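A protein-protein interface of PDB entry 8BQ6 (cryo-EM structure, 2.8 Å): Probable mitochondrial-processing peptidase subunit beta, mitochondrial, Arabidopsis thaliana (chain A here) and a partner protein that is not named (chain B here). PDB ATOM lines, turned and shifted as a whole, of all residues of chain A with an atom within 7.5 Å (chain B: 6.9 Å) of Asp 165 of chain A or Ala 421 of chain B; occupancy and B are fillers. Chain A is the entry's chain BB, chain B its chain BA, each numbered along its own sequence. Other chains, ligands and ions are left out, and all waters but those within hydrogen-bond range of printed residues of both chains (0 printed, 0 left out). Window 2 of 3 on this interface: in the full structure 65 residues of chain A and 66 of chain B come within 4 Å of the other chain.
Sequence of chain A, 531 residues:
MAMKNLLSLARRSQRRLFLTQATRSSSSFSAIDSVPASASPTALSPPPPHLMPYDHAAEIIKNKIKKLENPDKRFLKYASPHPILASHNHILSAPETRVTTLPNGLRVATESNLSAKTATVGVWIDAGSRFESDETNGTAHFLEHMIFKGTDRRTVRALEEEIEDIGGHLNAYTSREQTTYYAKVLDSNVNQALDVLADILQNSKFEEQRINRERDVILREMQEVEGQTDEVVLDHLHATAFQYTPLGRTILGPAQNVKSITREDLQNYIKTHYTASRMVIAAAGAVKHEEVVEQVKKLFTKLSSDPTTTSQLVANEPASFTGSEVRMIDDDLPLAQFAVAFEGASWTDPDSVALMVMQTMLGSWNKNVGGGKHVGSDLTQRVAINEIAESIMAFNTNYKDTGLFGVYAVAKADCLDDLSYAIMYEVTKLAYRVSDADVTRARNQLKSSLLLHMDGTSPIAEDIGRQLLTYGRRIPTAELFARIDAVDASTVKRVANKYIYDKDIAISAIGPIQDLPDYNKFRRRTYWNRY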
ATOM      1  N   ALA A 158     -22.947 -11.667 -23.494  1.00  0.00           N
ATOM      2  CA  ALA A 158     -21.600 -12.105 -23.846  1.00  0.00           C
ATOM      3  C   ALA A 158     -20.891 -11.099 -24.740  1.00  0.00           C
ATOM      4  O   ALA A 158     -19.676 -10.900 -24.636  1.00  0.00           O
ATOM      5  CB  ALA A 158     -21.672 -13.473 -24.529  1.00  0.00           C
ATOM      6  N   LEU A 159     -21.648 -10.450 -25.626  1.00  0.00           N
ATOM      7  CA  LEU A 159     -21.075  -9.411 -26.472  1.00  0.00           C
ATOM      8  C   LEU A 159     -20.619  -8.211 -25.649  1.00  0.00           C
ATOM      9  O   LEU A 159     -19.548  -7.650 -25.905  1.00  0.00           O
ATOM     10  CB  LEU A 159     -22.089  -8.985 -27.534  1.00  0.00           C
ATOM     11  CG  LEU A 159     -21.727  -7.745 -28.352  1.00  0.00           C
ATOM     12  CD1 LEU A 159     -20.496  -7.999 -29.197  1.00  0.00           C
ATOM     13  CD2 LEU A 159     -22.887  -7.314 -29.223  1.00  0.00           C
ATOM     14  N   GLU A 160     -21.407  -7.808 -24.649  1.00  0.00           N
ATOM     15  CA  GLU A 160     -21.110  -6.561 -23.952  1.00  0.00           C
ATOM     16  C   GLU A 160     -20.097  -6.779 -22.831  1.00  0.00           C
ATOM     17  O   GLU A 160     -19.301  -5.884 -22.525  1.00  0.00           O
ATOM     18  CB  GLU A 160     -22.406  -5.932 -23.433  1.00  0.00           C
ATOM     19  CG  GLU A 160     -22.207  -4.573 -22.745  1.00  0.00           C
ATOM     20  CD  GLU A 160     -23.500  -3.931 -22.274  1.00  0.00           C
ATOM     21  OE1 GLU A 160     -24.573  -4.547 -22.441  1.00  0.00           O
ATOM     22  OE2 GLU A 160     -23.438  -2.836 -21.688  1.00  0.00           O
ATOM     23  N   GLU A 161     -20.089  -7.968 -22.218  1.00  0.00           N
ATOM     24  CA  GLU A 161     -19.007  -8.279 -21.289  1.00  0.00           C
ATOM     25  C   GLU A 161     -17.668  -8.313 -22.012  1.00  0.00           C
ATOM     26  O   GLU A 161     -16.635  -7.942 -21.444  1.00  0.00           O
ATOM     27  CB  GLU A 161     -19.246  -9.614 -20.573  1.00  0.00           C
ATOM     28  CG  GLU A 161     -20.683 -10.097 -20.501  1.00  0.00           C
ATOM     29  CD  GLU A 161     -20.819 -11.444 -19.803  1.00  0.00           C
ATOM     30  OE1 GLU A 161     -20.660 -12.488 -20.474  1.00  0.00           O
ATOM     31  OE2 GLU A 161     -21.102 -11.462 -18.586  1.00  0.00           O
ATOM     32  N   GLU A 162     -17.666  -8.754 -23.271  1.00  0.00           N
ATOM     33  CA  GLU A 162     -16.421  -8.823 -24.023  1.00  0.00           C
ATOM     34  C   GLU A 162     -15.930  -7.439 -24.428  1.00  0.00           C
ATOM     35  O   GLU A 162     -14.725  -7.169 -24.369  1.00  0.00           O
ATOM     36  CB  GLU A 162     -16.606  -9.710 -25.250  1.00  0.00           C
ATOM     37  CG  GLU A 162     -15.595  -9.470 -26.338  1.00  0.00           C
ATOM     38  CD  GLU A 162     -15.769 -10.421 -27.496  1.00  0.00           C
ATOM     39  OE1 GLU A 162     -16.923 -10.803 -27.784  1.00  0.00           O
ATOM     40  OE2 GLU A 162     -14.750 -10.794 -28.110  1.00  0.00           O
ATOM     41  N   ILE A 163     -16.840  -6.554 -24.835  1.00  0.00           N
ATOM     42  CA  ILE A 163     -16.453  -5.183 -25.154  1.00  0.00           C
ATOM     43  C   ILE A 163     -15.906  -4.488 -23.915  1.00  0.00           C
ATOM     44  O   ILE A 163     -14.942  -3.716 -23.988  1.00  0.00           O
ATOM     45  CB  ILE A 163     -17.648  -4.425 -25.763  1.00  0.00           C
ATOM     46  CG1 ILE A 163     -18.039  -5.054 -27.100  1.00  0.00           C
ATOM     47  CG2 ILE A 163     -17.320  -2.958 -25.959  1.00  0.00           C
ATOM     48  CD1 ILE A 163     -16.865  -5.260 -28.031  1.00  0.00           C
ATOM     49  N   GLU A 164     -16.500  -4.763 -22.751  1.00  0.00           N
ATOM     50  CA  GLU A 164     -16.033  -4.139 -21.520  1.00  0.00           C
ATOM     51  C   GLU A 164     -14.711  -4.726 -21.047  1.00  0.00           C
ATOM     52  O   GLU A 164     -13.849  -3.985 -20.559  1.00  0.00           O
ATOM     53  CB  GLU A 164     -17.091  -4.274 -20.432  1.00  0.00           C
ATOM     54  CG  GLU A 164     -18.280  -3.372 -20.645  1.00  0.00           C
ATOM     55  CD  GLU A 164     -19.368  -3.610 -19.630  1.00  0.00           C
ATOM     56  OE1 GLU A 164     -19.630  -4.786 -19.309  1.00  0.00           O
ATOM     57  OE2 GLU A 164     -19.964  -2.620 -19.160  1.00  0.00           O
ATOM     58  N   ASP A 165     -14.532  -6.044 -21.175  1.00  0.00           N
ATOM     59  CA  ASP A 165     -13.283  -6.670 -20.752  1.00  0.00           C
ATOM     60  C   ASP A 165     -12.089  -6.067 -21.477  1.00  0.00           C
ATOM     61  O   ASP A 165     -11.014  -5.904 -20.887  1.00  0.00           O
ATOM     62  CB  ASP A 165     -13.346  -8.177 -20.986  1.00  0.00           C
ATOM     63  CG  ASP A 165     -14.104  -8.901 -19.896  1.00  0.00           C
ATOM     64  OD1 ASP A 165     -14.751  -8.217 -19.076  1.00  0.00           O
ATOM     65  OD2 ASP A 165     -14.059 -10.148 -19.861  1.00  0.00           O
ATOM     66  N   ILE A 166     -12.256  -5.728 -22.757  1.00  0.00           N
ATOM     67  CA  ILE A 166     -11.192  -5.051 -23.492  1.00  0.00           C
ATOM     68  C   ILE A 166     -11.266  -3.539 -23.365  1.00  0.00           C
ATOM     69  O   ILE A 166     -10.364  -2.842 -23.843  1.00  0.00           O
ATOM     70  CB  ILE A 166     -11.234  -5.463 -24.974  1.00  0.00           C
ATOM     71  CG1 ILE A 166     -12.541  -5.007 -25.616  1.00  0.00           C
ATOM     72  CG2 ILE A 166     -11.114  -6.964 -25.096  1.00  0.00           C
ATOM     73  CD1 ILE A 166     -12.619  -5.289 -27.091  1.00  0.00           C
ATOM     74  N   GLY A 167     -12.307  -3.012 -22.724  1.00  0.00           N
ATOM     75  CA  GLY A 167     -12.446  -1.577 -22.581  1.00  0.00           C
ATOM     76  C   GLY A 167     -12.801  -0.849 -23.853  1.00  0.00           C
ATOM     77  O   GLY A 167     -12.556   0.357 -23.954  1.00  0.00           O
ATOM     78  N   GLY A 168     -13.374  -1.544 -24.832  1.00  0.00           N
ATOM     79  CA  GLY A 168     -13.695  -0.955 -26.112  1.00  0.00           C
ATOM     80  C   GLY A 168     -15.029  -0.234 -26.116  1.00  0.00           C
ATOM     81  O   GLY A 168     -15.742  -0.158 -25.113  1.00  0.00           O
ATOM     82  N   LEU A 186      -8.158  -0.723 -28.155  1.00  0.00           N
ATOM     83  CA  LEU A 186      -6.716  -0.605 -28.040  1.00  0.00           C
ATOM     84  C   LEU A 186      -6.027  -1.339 -29.185  1.00  0.00           C
ATOM     85  O   LEU A 186      -6.622  -2.176 -29.868  1.00  0.00           O
ATOM     86  CB  LEU A 186      -6.237  -1.160 -26.702  1.00  0.00           C
ATOM     87  CG  LEU A 186      -6.535  -0.317 -25.465  1.00  0.00           C
ATOM     88  CD1 LEU A 186      -6.000  -1.017 -24.243  1.00  0.00           C
ATOM     89  CD2 LEU A 186      -5.914   1.061 -25.600  1.00  0.00           C
ATOM     90  N   ASN A 189      -6.184  -5.143 -29.713  1.00  0.00           N
ATOM     91  CA  ASN A 189      -7.510  -5.748 -29.793  1.00  0.00           C
ATOM     92  C   ASN A 189      -8.230  -5.440 -31.103  1.00  0.00           C
ATOM     93  O   ASN A 189      -9.463  -5.472 -31.147  1.00  0.00           O
ATOM     94  CB  ASN A 189      -8.367  -5.305 -28.608  1.00  0.00           C
ATOM     95  CG  ASN A 189      -7.675  -5.525 -27.285  1.00  0.00           C
ATOM     96  OD1 ASN A 189      -6.591  -4.996 -27.045  1.00  0.00           O
ATOM     97  ND2 ASN A 189      -8.287  -6.321 -26.423  1.00  0.00           N
ATOM     98  N   GLN A 192      -9.874  -8.729 -32.538  1.00  0.00           N
ATOM     99  CA  GLN A 192     -11.097  -9.046 -31.811  1.00  0.00           C
ATOM    100  C   GLN A 192     -12.251  -8.159 -32.262  1.00  0.00           C
ATOM    101  O   GLN A 192     -13.383  -8.632 -32.410  1.00  0.00           O
ATOM    102  CB  GLN A 192     -10.860  -8.905 -30.312  1.00  0.00           C
ATOM    103  CG  GLN A 192     -11.780  -9.752 -29.468  1.00  0.00           C
ATOM    104  CD  GLN A 192     -11.445  -9.652 -28.002  1.00  0.00           C
ATOM    105  OE1 GLN A 192     -10.352  -9.230 -27.633  1.00  0.00           O
ATOM    106  NE2 GLN A 192     -12.391 -10.028 -27.152  1.00  0.00           N
ATOM    107  N   ALA B 414     -14.433  -9.932 -12.229  1.00  0.00           N
ATOM    108  CA  ALA B 414     -14.922  -9.553 -13.576  1.00  0.00           C
ATOM    109  C   ALA B 414     -15.329  -8.074 -13.588  1.00  0.00           C
ATOM    110  O   ALA B 414     -14.956  -7.383 -14.542  1.00  0.00           O
ATOM    111  CB  ALA B 414     -16.069 -10.439 -13.974  1.00  0.00           C
ATOM    112  N   HIS B 415     -16.047  -7.615 -12.560  1.00  0.00           N
ATOM    113  CA  HIS B 415     -16.462  -6.189 -12.473  1.00  0.00           C
ATOM    114  C   HIS B 415     -15.232  -5.299 -12.274  1.00  0.00           C
ATOM    115  O   HIS B 415     -15.180  -4.239 -12.925  1.00  0.00           O
ATOM    116  CB  HIS B 415     -17.515  -6.003 -11.378  1.00  0.00           C
ATOM    117  CG  HIS B 415     -18.908  -5.978 -11.906  1.00  0.00           C
ATOM    118  ND1 HIS B 415     -19.627  -4.806 -12.031  1.00  0.00           N
ATOM    119  CD2 HIS B 415     -19.711  -6.967 -12.356  1.00  0.00           C
ATOM    120  CE1 HIS B 415     -20.818  -5.076 -12.524  1.00  0.00           C
ATOM    121  NE2 HIS B 415     -20.895  -6.395 -12.734  1.00  0.00           N
ATOM    122  N   LEU B 416     -14.284  -5.717 -11.424  1.00  0.00           N
ATOM    123  CA  LEU B 416     -13.042  -4.936 -11.171  1.00  0.00           C
ATOM    124  C   LEU B 416     -12.208  -4.848 -12.454  1.00  0.00           C
ATOM    125  O   LEU B 416     -11.738  -3.746 -12.763  1.00  0.00           O
ATOM    126  CB  LEU B 416     -12.254  -5.587 -10.027  1.00  0.00           C
ATOM    127  CG  LEU B 416     -10.909  -4.951  -9.681  1.00  0.00           C
ATOM    128  CD1 LEU B 416     -11.091  -3.525  -9.193  1.00  0.00           C
ATOM    129  CD2 LEU B 416     -10.170  -5.778  -8.642  1.00  0.00           C
ATOM    130  N   ASP B 417     -12.051  -5.958 -13.181  1.00  0.00           N
ATOM    131  CA  ASP B 417     -11.271  -5.962 -14.421  1.00  0.00           C
ATOM    132  C   ASP B 417     -11.917  -5.090 -15.489  1.00  0.00           C
ATOM    133  O   ASP B 417     -11.217  -4.439 -16.275  1.00  0.00           O
ATOM    134  CB  ASP B 417     -11.088  -7.383 -14.946  1.00  0.00           C
ATOM    135  CG  ASP B 417      -9.683  -7.898 -14.725  1.00  0.00           C
ATOM    136  OD1 ASP B 417      -9.376  -9.029 -15.155  1.00  0.00           O
ATOM    137  OD2 ASP B 417      -8.886  -7.161 -14.106  1.00  0.00           O
ATOM    138  N   ARG B 418     -13.248  -5.087 -15.557  1.00  0.00           N
ATOM    139  CA  ARG B 418     -13.925  -4.221 -16.513  1.00  0.00           C
ATOM    140  C   ARG B 418     -13.662  -2.756 -16.203  1.00  0.00           C
ATOM    141  O   ARG B 418     -13.396  -1.958 -17.111  1.00  0.00           O
ATOM    142  CB  ARG B 418     -15.421  -4.514 -16.514  1.00  0.00           C
ATOM    143  CG  ARG B 418     -15.788  -5.749 -17.298  1.00  0.00           C
ATOM    144  CD  ARG B 418     -17.243  -6.090 -17.111  1.00  0.00           C
ATOM    145  NE  ARG B 418     -17.469  -7.527 -17.166  1.00  0.00           N
ATOM    146  CZ  ARG B 418     -18.558  -8.130 -16.714  1.00  0.00           C
ATOM    147  NH1 ARG B 418     -19.530  -7.450 -16.127  1.00  0.00           N
ATOM    148  NH2 ARG B 418     -18.675  -9.447 -16.851  1.00  0.00           N
ATOM    149  N   ALA B 419     -13.719  -2.385 -14.923  1.00  0.00           N
ATOM    150  CA  ALA B 419     -13.434  -1.007 -14.543  1.00  0.00           C
ATOM    151  C   ALA B 419     -11.964  -0.657 -14.766  1.00  0.00           C
ATOM    152  O   ALA B 419     -11.643   0.488 -15.100  1.00  0.00           O
ATOM    153  CB  ALA B 419     -13.838  -0.767 -13.090  1.00  0.00           C
ATOM    154  N   LYS B 420     -11.055  -1.621 -14.580  1.00  0.00           N
ATOM    155  CA  LYS B 420      -9.643  -1.363 -14.871  1.00  0.00           C
ATOM    156  C   LYS B 420      -9.411  -1.128 -16.356  1.00  0.00           C
ATOM    157  O   LYS B 420      -8.649  -0.234 -16.741  1.00  0.00           O
ATOM    158  CB  LYS B 420      -8.758  -2.518 -14.411  1.00  0.00           C
ATOM    159  CG  LYS B 420      -8.527  -2.634 -12.939  1.00  0.00           C
ATOM    160  CD  LYS B 420      -7.334  -3.528 -12.707  1.00  0.00           C
ATOM    161  CE  LYS B 420      -7.292  -3.995 -11.283  1.00  0.00           C
ATOM    162  NZ  LYS B 420      -6.621  -5.315 -11.167  1.00  0.00           N
ATOM    163  N   ALA B 421     -10.003  -1.970 -17.204  1.00  0.00           N
ATOM    164  CA  ALA B 421      -9.821  -1.798 -18.640  1.00  0.00           C
ATOM    165  C   ALA B 421     -10.478  -0.513 -19.116  1.00  0.00           C
ATOM    166  O   ALA B 421      -9.920   0.208 -19.952  1.00  0.00           O
ATOM    167  CB  ALA B 421     -10.380  -3.001 -19.396  1.00  0.00           C
ATOM    168  N   ALA B 422     -11.663  -0.209 -18.585  1.00  0.00           N
ATOM    169  CA  ALA B 422     -12.333   1.041 -18.924  1.00  0.00           C
ATOM    170  C   ALA B 422     -11.495   2.239 -18.508  1.00  0.00           C
ATOM    171  O   ALA B 422     -11.441   3.246 -19.222  1.00  0.00           O
ATOM    172  CB  ALA B 422     -13.708   1.096 -18.261  1.00  0.00           C
ATOM    173  N   THR B 423     -10.843   2.151 -17.348  1.00  0.00           N
ATOM    174  CA  THR B 423     -10.013   3.256 -16.882  1.00  0.00           C
ATOM    175  C   THR B 423      -8.781   3.422 -17.761  1.00  0.00           C
ATOM    176  O   THR B 423      -8.457   4.536 -18.188  1.00  0.00           O
ATOM    177  CB  THR B 423      -9.625   3.031 -15.418  1.00  0.00           C
ATOM    178  OG1 THR B 423     -10.754   3.311 -14.582  1.00  0.00           O
ATOM    179  CG2 THR B 423      -8.468   3.935 -15.016  1.00  0.00           C
ATOM    180  N   LYS B 424      -8.089   2.320 -18.064  1.00  0.00           N
ATOM    181  CA  LYS B 424      -6.865   2.417 -18.854  1.00  0.00           C
ATOM    182  C   LYS B 424      -7.157   2.874 -20.280  1.00  0.00           C
ATOM    183  O   LYS B 424      -6.390   3.656 -20.856  1.00  0.00           O
ATOM    184  CB  LYS B 424      -6.129   1.077 -18.855  1.00  0.00           C
ATOM    185  CG  LYS B 424      -5.287   0.834 -20.094  1.00  0.00           C
ATOM    186  CD  LYS B 424      -5.071  -0.644 -20.343  1.00  0.00           C
ATOM    187  CE  LYS B 424      -3.927  -0.873 -21.315  1.00  0.00           C
ATOM    188  NZ  LYS B 424      -2.605  -0.812 -20.644  1.00  0.00           N
ATOM    189  N   SER B 425      -8.257   2.396 -20.872  1.00  0.00           N
ATOM    190  CA  SER B 425      -8.590   2.797 -22.237  1.00  0.00           C
ATOM    191  C   SER B 425      -8.941   4.274 -22.323  1.00  0.00           C
ATOM    192  O   SER B 425      -8.532   4.952 -23.274  1.00  0.00           O
ATOM    193  CB  SER B 425      -9.751   1.962 -22.774  1.00  0.00           C
ATOM    194  OG  SER B 425     -10.950   2.260 -22.080  1.00  0.00           O
ATOM    195  N   ALA B 426      -9.695   4.785 -21.347  1.00  0.00           N
ATOM    196  CA  ALA B 426     -10.128   6.179 -21.361  1.00  0.00           C
ATOM    197  C   ALA B 426      -8.948   7.140 -21.342  1.00  0.00           C
ATOM    198  O   ALA B 426      -8.936   8.121 -22.094  1.00  0.00           O
ATOM    199  CB  ALA B 426     -11.043   6.453 -20.169  1.00  0.00           C
ATOM    200  N   VAL B 461      -2.612   1.234 -12.248  1.00  0.00           N
ATOM    201  CA  VAL B 461      -3.971   0.753 -12.480  1.00  0.00           C
ATOM    202  C   VAL B 461      -4.008  -0.769 -12.431  1.00  0.00           C
ATOM    203  O   VAL B 461      -4.785  -1.363 -11.675  1.00  0.00           O
ATOM    204  CB  VAL B 461      -4.512   1.289 -13.817  1.00  0.00           C
ATOM    205  CG1 VAL B 461      -5.787   0.558 -14.203  1.00  0.00           C
ATOM    206  CG2 VAL B 461      -4.763   2.779 -13.729  1.00  0.00           C
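O of Ala 421 of chain B lies within hydrogen-bond range of OG of Ser 425 of chain B, at 3.1 Å. The side-chain hydroxyl (OG) of Ser 425 of chain B is in hydrogen-bond range of the backbone carbonyl oxygen (O) of Ala 422 of chain B (3.1 Å).
The guanidinium group (NH2) of Arg 418 of chain B lies within salt-bridge range of the side-chain carboxylate (OE2) of Glu 161 of chain A (3.6 Å). The side-chain carboxylate of Asp 165 of chain A lies within salt-bridge range of the guanidinium group of Arg 418 of chain B, 3.4 Å away. OG of Ser 425 of chain B lies within hydrogen-bond range of O of Gly 167 of chain A (3.1 Å).
OE1 of Glu 164 of chain A touches CD of Arg 418 of chain B (3.5 Å). Ala 421 of chain B touches Glu 164 of chain A (CB to O, 3.8 Å). Ala 421 of chain B touches Asp 165 of chain A. N of Gly 167 of chain A touches CB of Ala 421 of chain B, 3.8 Å away. CD1 of Leu 186 of chain A touches CE of Lys 424 of chain B (3.6 Å).
Of chain B, only Arg 418 and Ala 421 come within 4 Å of Asp 165 of chain A. Of chain A, only Glu 164, Asp 165 and Gly 167 come within 4 Å of Ala 421 of chain B. Printed residues of chain B within 4 Å of Glu 161 of chain A: Arg 418. Of the printed residues of chain A, Lys 424 of chain B touches Leu 186 (3.6 Å). Printed residues of chain B within 4 Å of Leu 186 of chain A: Lys 424. Printed residues of chain A within 4 Å of Arg 418 of chain B: Glu 161, Glu 164 and Asp 165. Printed residues of chain B within 4 Å of Gly 167 of chain A: Ala 421 (3.8 Å) and Ser 425 (3.1 Å). Leu 416 of chain B touches none of the printed residues of chain A. The nearest residue of chain A that does not touch Ala 421 of chain B is Ile 166 of chain A (4.1 Å).
Of the 14 printed residues of chain A, 5 touch a printed residue of chain B. Printed residues of chain A that touch a printed residue of chain B: Glu 161, Glu 164, Asp 165, Gly 167 and Leu 186. Hydrophobic or aromatic side chains of chain A within 4 Å of the printed part of chain B: Leu 186. Of the 14 printed residues of chain B, 4 touch a printed residue of chain A. Among the printed residues, Asp or Glu carboxylates within 4 Å of a Lys or Arg side-chain nitrogen of the other chain: Glu 161 of chain A with Arg 418 of chain B and Asp 165 of chain A with Arg 418 of chain B.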
